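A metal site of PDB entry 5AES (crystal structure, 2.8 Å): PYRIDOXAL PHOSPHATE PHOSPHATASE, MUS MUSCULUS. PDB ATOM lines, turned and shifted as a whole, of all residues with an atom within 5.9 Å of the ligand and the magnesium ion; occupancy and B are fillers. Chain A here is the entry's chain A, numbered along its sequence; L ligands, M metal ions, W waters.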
ATOM      1  N   ASP A  26       8.822  23.519 -23.024  1.00  0.00           N
ATOM      2  CA  ASP A  26       7.964  24.429 -23.753  1.00  0.00           C
ATOM      3  C   ASP A  26       8.924  25.319 -24.530  1.00  0.00           C
ATOM      4  O   ASP A  26      10.095  25.441 -24.155  1.00  0.00           O
ATOM      5  CB  ASP A  26       7.107  25.271 -22.812  1.00  0.00           C
ATOM      6  CG  ASP A  26       6.356  26.385 -23.536  1.00  0.00           C
ATOM      7  OD1 ASP A  26       5.683  26.117 -24.548  1.00  0.00           O
ATOM      8  OD2 ASP A  26       6.469  27.559 -23.109  1.00  0.00           O
ATOM      9  N   CYS A  27       8.454  25.939 -25.613  1.00  0.00           N
ATOM     10  CA  CYS A  27       9.345  26.702 -26.481  1.00  0.00           C
ATOM     11  C   CYS A  27       9.367  28.197 -26.190  1.00  0.00           C
ATOM     12  O   CYS A  27      10.359  28.730 -25.698  1.00  0.00           O
ATOM     13  CB  CYS A  27       8.975  26.470 -27.940  1.00  0.00           C
ATOM     14  SG  CYS A  27       9.096  24.754 -28.431  1.00  0.00           S
ATOM     15  N   ASP A  28       8.268  28.877 -26.510  1.00  0.00           N
ATOM     16  CA  ASP A  28       8.200  30.316 -26.312  1.00  0.00           C
ATOM     17  C   ASP A  28       8.295  30.660 -24.836  1.00  0.00           C
ATOM     18  O   ASP A  28       7.532  30.145 -24.004  1.00  0.00           O
ATOM     19  CB  ASP A  28       6.916  30.894 -26.912  1.00  0.00           C
ATOM     20  CG  ASP A  28       6.992  31.027 -28.424  1.00  0.00           C
ATOM     21  OD1 ASP A  28       7.567  32.038 -28.897  1.00  0.00           O
ATOM     22  OD2 ASP A  28       6.481  30.130 -29.143  1.00  0.00           O
ATOM     23  N   GLY A  29       9.231  31.536 -24.506  1.00  0.00           N
ATOM     24  CA  GLY A  29       9.456  31.980 -23.146  1.00  0.00           C
ATOM     25  C   GLY A  29      10.489  31.128 -22.437  1.00  0.00           C
ATOM     26  O   GLY A  29      10.900  31.428 -21.333  1.00  0.00           O
ATOM     27  N   VAL A  30      10.930  30.062 -23.102  1.00  0.00           N
ATOM     28  CA  VAL A  30      11.876  29.112 -22.516  1.00  0.00           C
ATOM     29  C   VAL A  30      13.149  29.025 -23.344  1.00  0.00           C
ATOM     30  O   VAL A  30      14.248  29.238 -22.845  1.00  0.00           O
ATOM     31  CB  VAL A  30      11.237  27.722 -22.417  1.00  0.00           C
ATOM     32  CG1 VAL A  30      12.177  26.739 -21.766  1.00  0.00           C
ATOM     33  CG2 VAL A  30       9.923  27.805 -21.661  1.00  0.00           C
ATOM     34  N   VAL A  58       7.184  21.067 -26.635  1.00  0.00           N
ATOM     35  CA  VAL A  58       5.760  21.356 -26.721  1.00  0.00           C
ATOM     36  C   VAL A  58       5.520  22.839 -26.920  1.00  0.00           C
ATOM     37  O   VAL A  58       6.271  23.674 -26.424  1.00  0.00           O
ATOM     38  CB  VAL A  58       5.003  20.932 -25.454  1.00  0.00           C
ATOM     39  CG1 VAL A  58       4.946  19.411 -25.337  1.00  0.00           C
ATOM     40  CG2 VAL A  58       5.657  21.564 -24.237  1.00  0.00           C
ATOM     41  N   SER A  59       4.473  23.173 -27.667  1.00  0.00           N
ATOM     42  CA  SER A  59       4.153  24.554 -27.943  1.00  0.00           C
ATOM     43  C   SER A  59       2.679  24.669 -28.239  1.00  0.00           C
ATOM     44  O   SER A  59       2.125  23.823 -28.936  1.00  0.00           O
ATOM     45  CB  SER A  59       4.982  25.045 -29.134  1.00  0.00           C
ATOM     46  OG  SER A  59       4.743  26.418 -29.368  1.00  0.00           O
ATOM     47  N   ASN A  60       2.042  25.704 -27.706  1.00  0.00           N
ATOM     48  CA  ASN A  60       0.651  25.974 -28.022  1.00  0.00           C
ATOM     49  C   ASN A  60       0.559  26.919 -29.220  1.00  0.00           C
ATOM     50  O   ASN A  60      -0.533  27.342 -29.625  1.00  0.00           O
ATOM     51  CB  ASN A  60      -0.079  26.533 -26.802  1.00  0.00           C
ATOM     52  CG  ASN A  60      -0.579  25.434 -25.862  1.00  0.00           C
ATOM     53  OD1 ASN A  60      -0.622  24.245 -26.229  1.00  0.00           O
ATOM     54  ND2 ASN A  60      -0.955  25.817 -24.650  1.00  0.00           N
ATOM     55  N   ASN A  61       1.708  27.216 -29.804  1.00  0.00           N
ATOM     56  CA  ASN A  61       1.758  28.016 -31.020  1.00  0.00           C
ATOM     57  C   ASN A  61       1.277  27.215 -32.224  1.00  0.00           C
ATOM     58  O   ASN A  61       1.853  26.182 -32.586  1.00  0.00           O
ATOM     59  CB  ASN A  61       3.175  28.531 -31.244  1.00  0.00           C
ATOM     60  CG  ASN A  61       3.230  29.655 -32.257  1.00  0.00           C
ATOM     61  OD1 ASN A  61       2.461  29.669 -33.208  1.00  0.00           O
ATOM     62  ND2 ASN A  61       4.114  30.614 -32.023  1.00  0.00           N
ATOM     63  N   SER A  62       0.202  27.689 -32.832  1.00  0.00           N
ATOM     64  CA  SER A  62      -0.417  27.021 -33.963  1.00  0.00           C
ATOM     65  C   SER A  62      -0.190  27.781 -35.261  1.00  0.00           C
ATOM     66  O   SER A  62      -0.978  27.690 -36.186  1.00  0.00           O
ATOM     67  CB  SER A  62      -1.917  26.861 -33.728  1.00  0.00           C
ATOM     68  OG  SER A  62      -2.560  28.096 -33.453  1.00  0.00           O
ATOM     69  N   ARG A  63       0.912  28.519 -35.310  1.00  0.00           N
ATOM     70  CA  ARG A  63       1.198  29.341 -36.477  1.00  0.00           C
ATOM     71  C   ARG A  63       2.108  28.634 -37.473  1.00  0.00           C
ATOM     72  O   ARG A  63       2.027  28.883 -38.675  1.00  0.00           O
ATOM     73  CB  ARG A  63       1.835  30.653 -36.030  1.00  0.00           C
ATOM     74  CG  ARG A  63       0.827  31.707 -35.612  1.00  0.00           C
ATOM     75  CD  ARG A  63       1.465  33.089 -35.487  1.00  0.00           C
ATOM     76  NE  ARG A  63       2.221  33.462 -36.682  1.00  0.00           N
ATOM     77  CZ  ARG A  63       2.633  34.693 -36.945  1.00  0.00           C
ATOM     78  NH1 ARG A  63       2.370  35.689 -36.110  1.00  0.00           N
ATOM     79  NH2 ARG A  63       3.327  34.929 -38.052  1.00  0.00           N
ATOM     80  N   TYR A 147      -5.174  30.075 -33.353  1.00  0.00           N
ATOM     81  CA  TYR A 147      -4.774  31.471 -33.389  1.00  0.00           C
ATOM     82  C   TYR A 147      -5.129  32.013 -34.770  1.00  0.00           C
ATOM     83  O   TYR A 147      -4.561  31.602 -35.767  1.00  0.00           O
ATOM     84  CB  TYR A 147      -3.266  31.603 -33.128  1.00  0.00           C
ATOM     85  CG  TYR A 147      -2.761  33.013 -33.079  1.00  0.00           C
ATOM     86  CD1 TYR A 147      -2.867  33.760 -31.921  1.00  0.00           C
ATOM     87  CD2 TYR A 147      -2.180  33.601 -34.190  1.00  0.00           C
ATOM     88  CE1 TYR A 147      -2.410  35.050 -31.868  1.00  0.00           C
ATOM     89  CE2 TYR A 147      -1.710  34.893 -34.139  1.00  0.00           C
ATOM     90  CZ  TYR A 147      -1.827  35.629 -32.975  1.00  0.00           C
ATOM     91  OH  TYR A 147      -1.372  36.932 -32.912  1.00  0.00           O
ATOM     92  N   ASP A 174      -5.783  25.243 -28.191  1.00  0.00           N
ATOM     93  CA  ASP A 174      -5.381  25.539 -26.819  1.00  0.00           C
ATOM     94  C   ASP A 174      -6.270  26.614 -26.213  1.00  0.00           C
ATOM     95  O   ASP A 174      -7.098  27.201 -26.921  1.00  0.00           O
ATOM     96  CB  ASP A 174      -3.942  26.038 -26.827  1.00  0.00           C
ATOM     97  CG  ASP A 174      -3.791  27.363 -27.529  1.00  0.00           C
ATOM     98  OD1 ASP A 174      -3.739  27.376 -28.781  1.00  0.00           O
ATOM     99  OD2 ASP A 174      -3.724  28.393 -26.832  1.00  0.00           O
ATOM    100  N   ASP A 176      -4.831  29.264 -24.260  1.00  0.00           N
ATOM    101  CA  ASP A 176      -3.995  30.374 -23.814  1.00  0.00           C
ATOM    102  C   ASP A 176      -4.726  31.676 -24.117  1.00  0.00           C
ATOM    103  O   ASP A 176      -5.090  31.927 -25.266  1.00  0.00           O
ATOM    104  CB  ASP A 176      -2.624  30.328 -24.475  1.00  0.00           C
ATOM    105  CG  ASP A 176      -1.733  29.221 -23.924  1.00  0.00           C
ATOM    106  OD1 ASP A 176      -2.199  28.420 -23.092  1.00  0.00           O
ATOM    107  OD2 ASP A 176      -0.560  29.162 -24.330  1.00  0.00           O
ATOM    108  N   HIS A 179      -0.816  36.505 -25.307  1.00  0.00           N
ATOM    109  CA  HIS A 179       0.629  36.301 -25.362  1.00  0.00           C
ATOM    110  C   HIS A 179       1.343  37.639 -25.416  1.00  0.00           C
ATOM    111  O   HIS A 179       0.852  38.579 -26.043  1.00  0.00           O
ATOM    112  CB  HIS A 179       1.018  35.443 -26.570  1.00  0.00           C
ATOM    113  CG  HIS A 179       0.300  34.137 -26.641  1.00  0.00           C
ATOM    114  ND1 HIS A 179       0.632  33.066 -25.839  1.00  0.00           N
ATOM    115  CD2 HIS A 179      -0.749  33.725 -27.394  1.00  0.00           C
ATOM    116  CE1 HIS A 179      -0.178  32.052 -26.096  1.00  0.00           C
ATOM    117  NE2 HIS A 179      -1.018  32.431 -27.043  1.00  0.00           N
ATOM    118  N   PRO A 180       2.511  37.723 -24.777  1.00  0.00           N
ATOM    119  CA  PRO A 180       3.310  38.952 -24.797  1.00  0.00           C
ATOM    120  C   PRO A 180       4.065  39.085 -26.113  1.00  0.00           C
ATOM    121  O   PRO A 180       4.507  38.075 -26.654  1.00  0.00           O
ATOM    122  CB  PRO A 180       4.313  38.731 -23.673  1.00  0.00           C
ATOM    123  CG  PRO A 180       4.519  37.266 -23.675  1.00  0.00           C
ATOM    124  CD  PRO A 180       3.184  36.652 -24.033  1.00  0.00           C
ATOM    125  N   LEU A 181       4.209  40.307 -26.609  1.00  0.00           N
ATOM    126  CA  LEU A 181       4.986  40.560 -27.820  1.00  0.00           C
ATOM    127  C   LEU A 181       6.258  41.313 -27.457  1.00  0.00           C
ATOM    128  O   LEU A 181       6.442  41.726 -26.309  1.00  0.00           O
ATOM    129  CB  LEU A 181       4.179  41.361 -28.831  1.00  0.00           C
ATOM    130  CG  LEU A 181       2.872  40.728 -29.320  1.00  0.00           C
ATOM    131  CD1 LEU A 181       2.245  41.574 -30.423  1.00  0.00           C
ATOM    132  CD2 LEU A 181       3.097  39.301 -29.808  1.00  0.00           C
ATOM    133  N   THR A 187      -1.135  39.985 -27.467  1.00  0.00           N
ATOM    134  CA  THR A 187      -1.998  39.558 -28.547  1.00  0.00           C
ATOM    135  C   THR A 187      -2.990  38.549 -27.988  1.00  0.00           C
ATOM    136  O   THR A 187      -2.613  37.699 -27.182  1.00  0.00           O
ATOM    137  CB  THR A 187      -1.192  38.920 -29.705  1.00  0.00           C
ATOM    138  OG1 THR A 187      -2.087  38.582 -30.787  1.00  0.00           O
ATOM    139  CG2 THR A 187      -0.463  37.675 -29.241  1.00  0.00           C
ATOM    140  N   THR A 190      -5.740  31.801 -28.554  1.00  0.00           N
ATOM    141  CA  THR A 190      -6.825  30.913 -28.966  1.00  0.00           C
ATOM    142  C   THR A 190      -7.879  30.790 -27.872  1.00  0.00           C
ATOM    143  O   THR A 190      -9.056  30.593 -28.150  1.00  0.00           O
ATOM    144  CB  THR A 190      -6.282  29.517 -29.286  1.00  0.00           C
ATOM    145  OG1 THR A 190      -5.158  29.636 -30.164  1.00  0.00           O
ATOM    146  CG2 THR A 190      -7.371  28.655 -29.927  1.00  0.00           C
ATOM    147  N   LYS A 210      -1.606  22.037 -24.149  1.00  0.00           N
ATOM    148  CA  LYS A 210      -1.403  22.208 -22.714  1.00  0.00           C
ATOM    149  C   LYS A 210      -2.396  23.217 -22.158  1.00  0.00           C
ATOM    150  O   LYS A 210      -2.636  24.252 -22.787  1.00  0.00           O
ATOM    151  CB  LYS A 210      -0.018  22.763 -22.436  1.00  0.00           C
ATOM    152  CG  LYS A 210       1.130  21.969 -22.987  1.00  0.00           C
ATOM    153  CD  LYS A 210       2.407  22.789 -22.929  1.00  0.00           C
ATOM    154  CE  LYS A 210       2.382  23.920 -23.930  1.00  0.00           C
ATOM    155  NZ  LYS A 210       3.485  24.883 -23.685  1.00  0.00           N
ATOM    156  N   GLY A 234       8.763  24.873 -18.338  1.00  0.00           N
ATOM    157  CA  GLY A 234       7.975  25.895 -18.987  1.00  0.00           C
ATOM    158  C   GLY A 234       8.022  27.231 -18.274  1.00  0.00           C
ATOM    159  O   GLY A 234       8.582  27.345 -17.187  1.00  0.00           O
ATOM    160  N   ASP A 235       7.417  28.250 -18.876  1.00  0.00           N
ATOM    161  CA  ASP A 235       7.476  29.598 -18.351  1.00  0.00           C
ATOM    162  C   ASP A 235       6.103  30.081 -17.899  1.00  0.00           C
ATOM    163  O   ASP A 235       5.964  31.213 -17.414  1.00  0.00           O
ATOM    164  CB  ASP A 235       7.999  30.543 -19.431  1.00  0.00           C
ATOM    165  CG  ASP A 235       7.016  30.733 -20.561  1.00  0.00           C
ATOM    166  OD1 ASP A 235       6.614  29.722 -21.185  1.00  0.00           O
ATOM    167  OD2 ASP A 235       6.627  31.885 -20.821  1.00  0.00           O
ATOM    168  N   ARG A 236       5.080  29.251 -18.072  1.00  0.00           N
ATOM    169  CA  ARG A 236       3.711  29.642 -17.761  1.00  0.00           C
ATOM    170  C   ARG A 236       3.045  28.665 -16.793  1.00  0.00           C
ATOM    171  O   ARG A 236       3.024  27.461 -17.034  1.00  0.00           O
ATOM    172  CB  ARG A 236       2.898  29.763 -19.052  1.00  0.00           C
ATOM    173  CG  ARG A 236       1.651  30.622 -18.920  1.00  0.00           C
ATOM    174  CD  ARG A 236       1.183  31.088 -20.278  1.00  0.00           C
ATOM    175  NE  ARG A 236       0.152  32.122 -20.176  1.00  0.00           N
ATOM    176  CZ  ARG A 236      -0.254  32.881 -21.188  1.00  0.00           C
ATOM    177  NH1 ARG A 236       0.274  32.736 -22.389  1.00  0.00           N
ATOM    178  NH2 ARG A 236      -1.203  33.795 -20.987  1.00  0.00           N
ATOM    179  N   THR A 239      -0.507  26.905 -17.767  1.00  0.00           N
ATOM    180  CA  THR A 239      -0.517  25.983 -18.904  1.00  0.00           C
ATOM    181  C   THR A 239       0.595  24.946 -18.769  1.00  0.00           C
ATOM    182  O   THR A 239       0.326  23.743 -18.771  1.00  0.00           O
ATOM    183  CB  THR A 239      -0.359  26.699 -20.279  1.00  0.00           C
ATOM    184  OG1 THR A 239       1.025  26.871 -20.584  1.00  0.00           O
ATOM    185  CG2 THR A 239      -1.053  28.050 -20.286  1.00  0.00           C
ATOM    186  N   ASP A 240       1.840  25.395 -18.630  1.00  0.00           N
ATOM    187  CA  ASP A 240       2.997  24.496 -18.596  1.00  0.00           C
ATOM    188  C   ASP A 240       3.085  23.682 -17.303  1.00  0.00           C
ATOM    189  O   ASP A 240       3.250  22.463 -17.349  1.00  0.00           O
ATOM    190  CB  ASP A 240       4.289  25.288 -18.809  1.00  0.00           C
ATOM    191  CG  ASP A 240       4.312  26.033 -20.130  1.00  0.00           C
ATOM    192  OD1 ASP A 240       3.898  25.448 -21.142  1.00  0.00           O
ATOM    193  OD2 ASP A 240       4.748  27.212 -20.156  1.00  0.00           O
ATOM    194  N   VAL A 258       6.509  34.426 -19.367  1.00  0.00           N
ATOM    195  CA  VAL A 258       5.303  35.071 -18.854  1.00  0.00           C
ATOM    196  C   VAL A 258       5.231  35.150 -17.332  1.00  0.00           C
ATOM    197  O   VAL A 258       5.046  36.241 -16.774  1.00  0.00           O
ATOM    198  CB  VAL A 258       4.084  34.345 -19.361  1.00  0.00           C
ATOM    199  CG1 VAL A 258       2.830  34.921 -18.735  1.00  0.00           C
ATOM    200  CG2 VAL A 258       4.022  34.428 -20.888  1.00  0.00           C
HETATM  201  O1  LIG L   1       5.532  27.646 -26.666  1.00  0.00           O
HETATM  202  P1  LIG L   1       4.360  28.442 -26.031  1.00  0.00           P
HETATM  203  O2  LIG L   1       3.279  27.452 -25.510  1.00  0.00           O
HETATM  204  O3  LIG L   1       4.877  29.272 -24.893  1.00  0.00           O
HETATM  205  C1  LIG L   1       3.636  29.490 -27.323  1.00  0.00           C
HETATM  206  C2  LIG L   1       2.311  30.142 -27.106  1.00  0.00           C
HETATM  207  C3  LIG L   1       1.783  30.858 -28.304  1.00  0.00           C
HETATM  208  C4  LIG L   1       0.661  30.375 -28.964  1.00  0.00           C
HETATM  209  N1  LIG L   1       0.189  31.003 -30.050  1.00  0.00           N
HETATM  210  C5  LIG L   1       0.800  32.105 -30.507  1.00  0.00           C
HETATM  211  C6  LIG L   1       0.254  32.792 -31.715  1.00  0.00           C
HETATM  212  C7  LIG L   1       1.912  32.633 -29.902  1.00  0.00           C
HETATM  213  O4  LIG L   1       2.499  33.771 -30.424  1.00  0.00           O
HETATM  214  C8  LIG L   1       2.436  32.000 -28.773  1.00  0.00           C
HETATM  215  C9  LIG L   1       3.658  32.522 -28.075  1.00  0.00           C
HETATM  216  O5  LIG L   1       3.978  33.850 -28.246  1.00  0.00           O
HETATM  217 MG    MG M   1       5.752  29.506 -23.081  1.00  0.00          MG
HETATM  218  O   HOH W   1      -2.196  29.096 -30.820  1.00  0.00           O
HETATM  219  O   HOH W   2       4.031  28.821 -22.206  1.00  0.00           O
HETATM  220  O   HOH W   3       5.133  31.474 -23.001  1.00  0.00           O
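OG1 of Thr 187 sits at hydrogen-bond distance from OH of Tyr 147, 2.8 Å away. N of Thr 187 lies within hydrogen-bond range of O of His 179, at 2.8 Å. OG1 of Thr 239 is in hydrogen-bond range of OD1 of Asp 240. The backbone NH of Asp 235 lies within hydrogen-bond range of the side-chain carboxylate of Asp 240 (3.1 Å). The backbone NH (N) of Arg 63 sits at hydrogen-bond distance from the side-chain amide oxygen (OD1) of Asn 61 (2.9 Å). N of Tyr 147 is in hydrogen-bond range of OG of Ser 62 (3.3 Å). O of Val 58 is in hydrogen-bond range of N of Cys 27 (3.2 Å). The side-chain amide nitrogen (ND2) of Asn 60 is in hydrogen-bond range of the backbone carbonyl oxygen (O) of Lys 210 (3.0 Å).
Cys 27 touches the ligand (N to O1, 3.5 Å). Asn 61 touches the ligand. Arg 63 touches the ligand (CD to C6, 3.97 Å). Tyr 147 touches the ligand. CE1 of His 179 touches C3 of the ligand, 3.2 Å away. Of the 26 residues printed, 10 come within 4 Å of the ligand. The nearest printed residue that does not touch the ligand is Val 58 (4.05 Å).
An oxygen (O1) of the ligand lies within hydrogen-bond range of the side-chain hydroxyl (OG) of Ser 59 (3.1 Å). An oxygen (O2) of the ligand lies within salt-bridge range of the side-chain amino group (NZ) of Lys 210, 3.2 Å away. N of Asn 60 lies within hydrogen-bond range of O2 of the ligand. N of Asp 28 is in hydrogen-bond range of O1 of the ligand, 3.0 Å away.
The magnesium ion is bound by O3 of the ligand (2.0 Å), water W2 (2.0 Å), water W3 (2.1 Å), OD2 of Asp 26 (2.1 Å), OD1 of Asp 235 (2.1 Å) and O of Asp 28 (2.1 Å).
Merely in contact with the magnesium ion: Asp 240 (3.9 Å).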
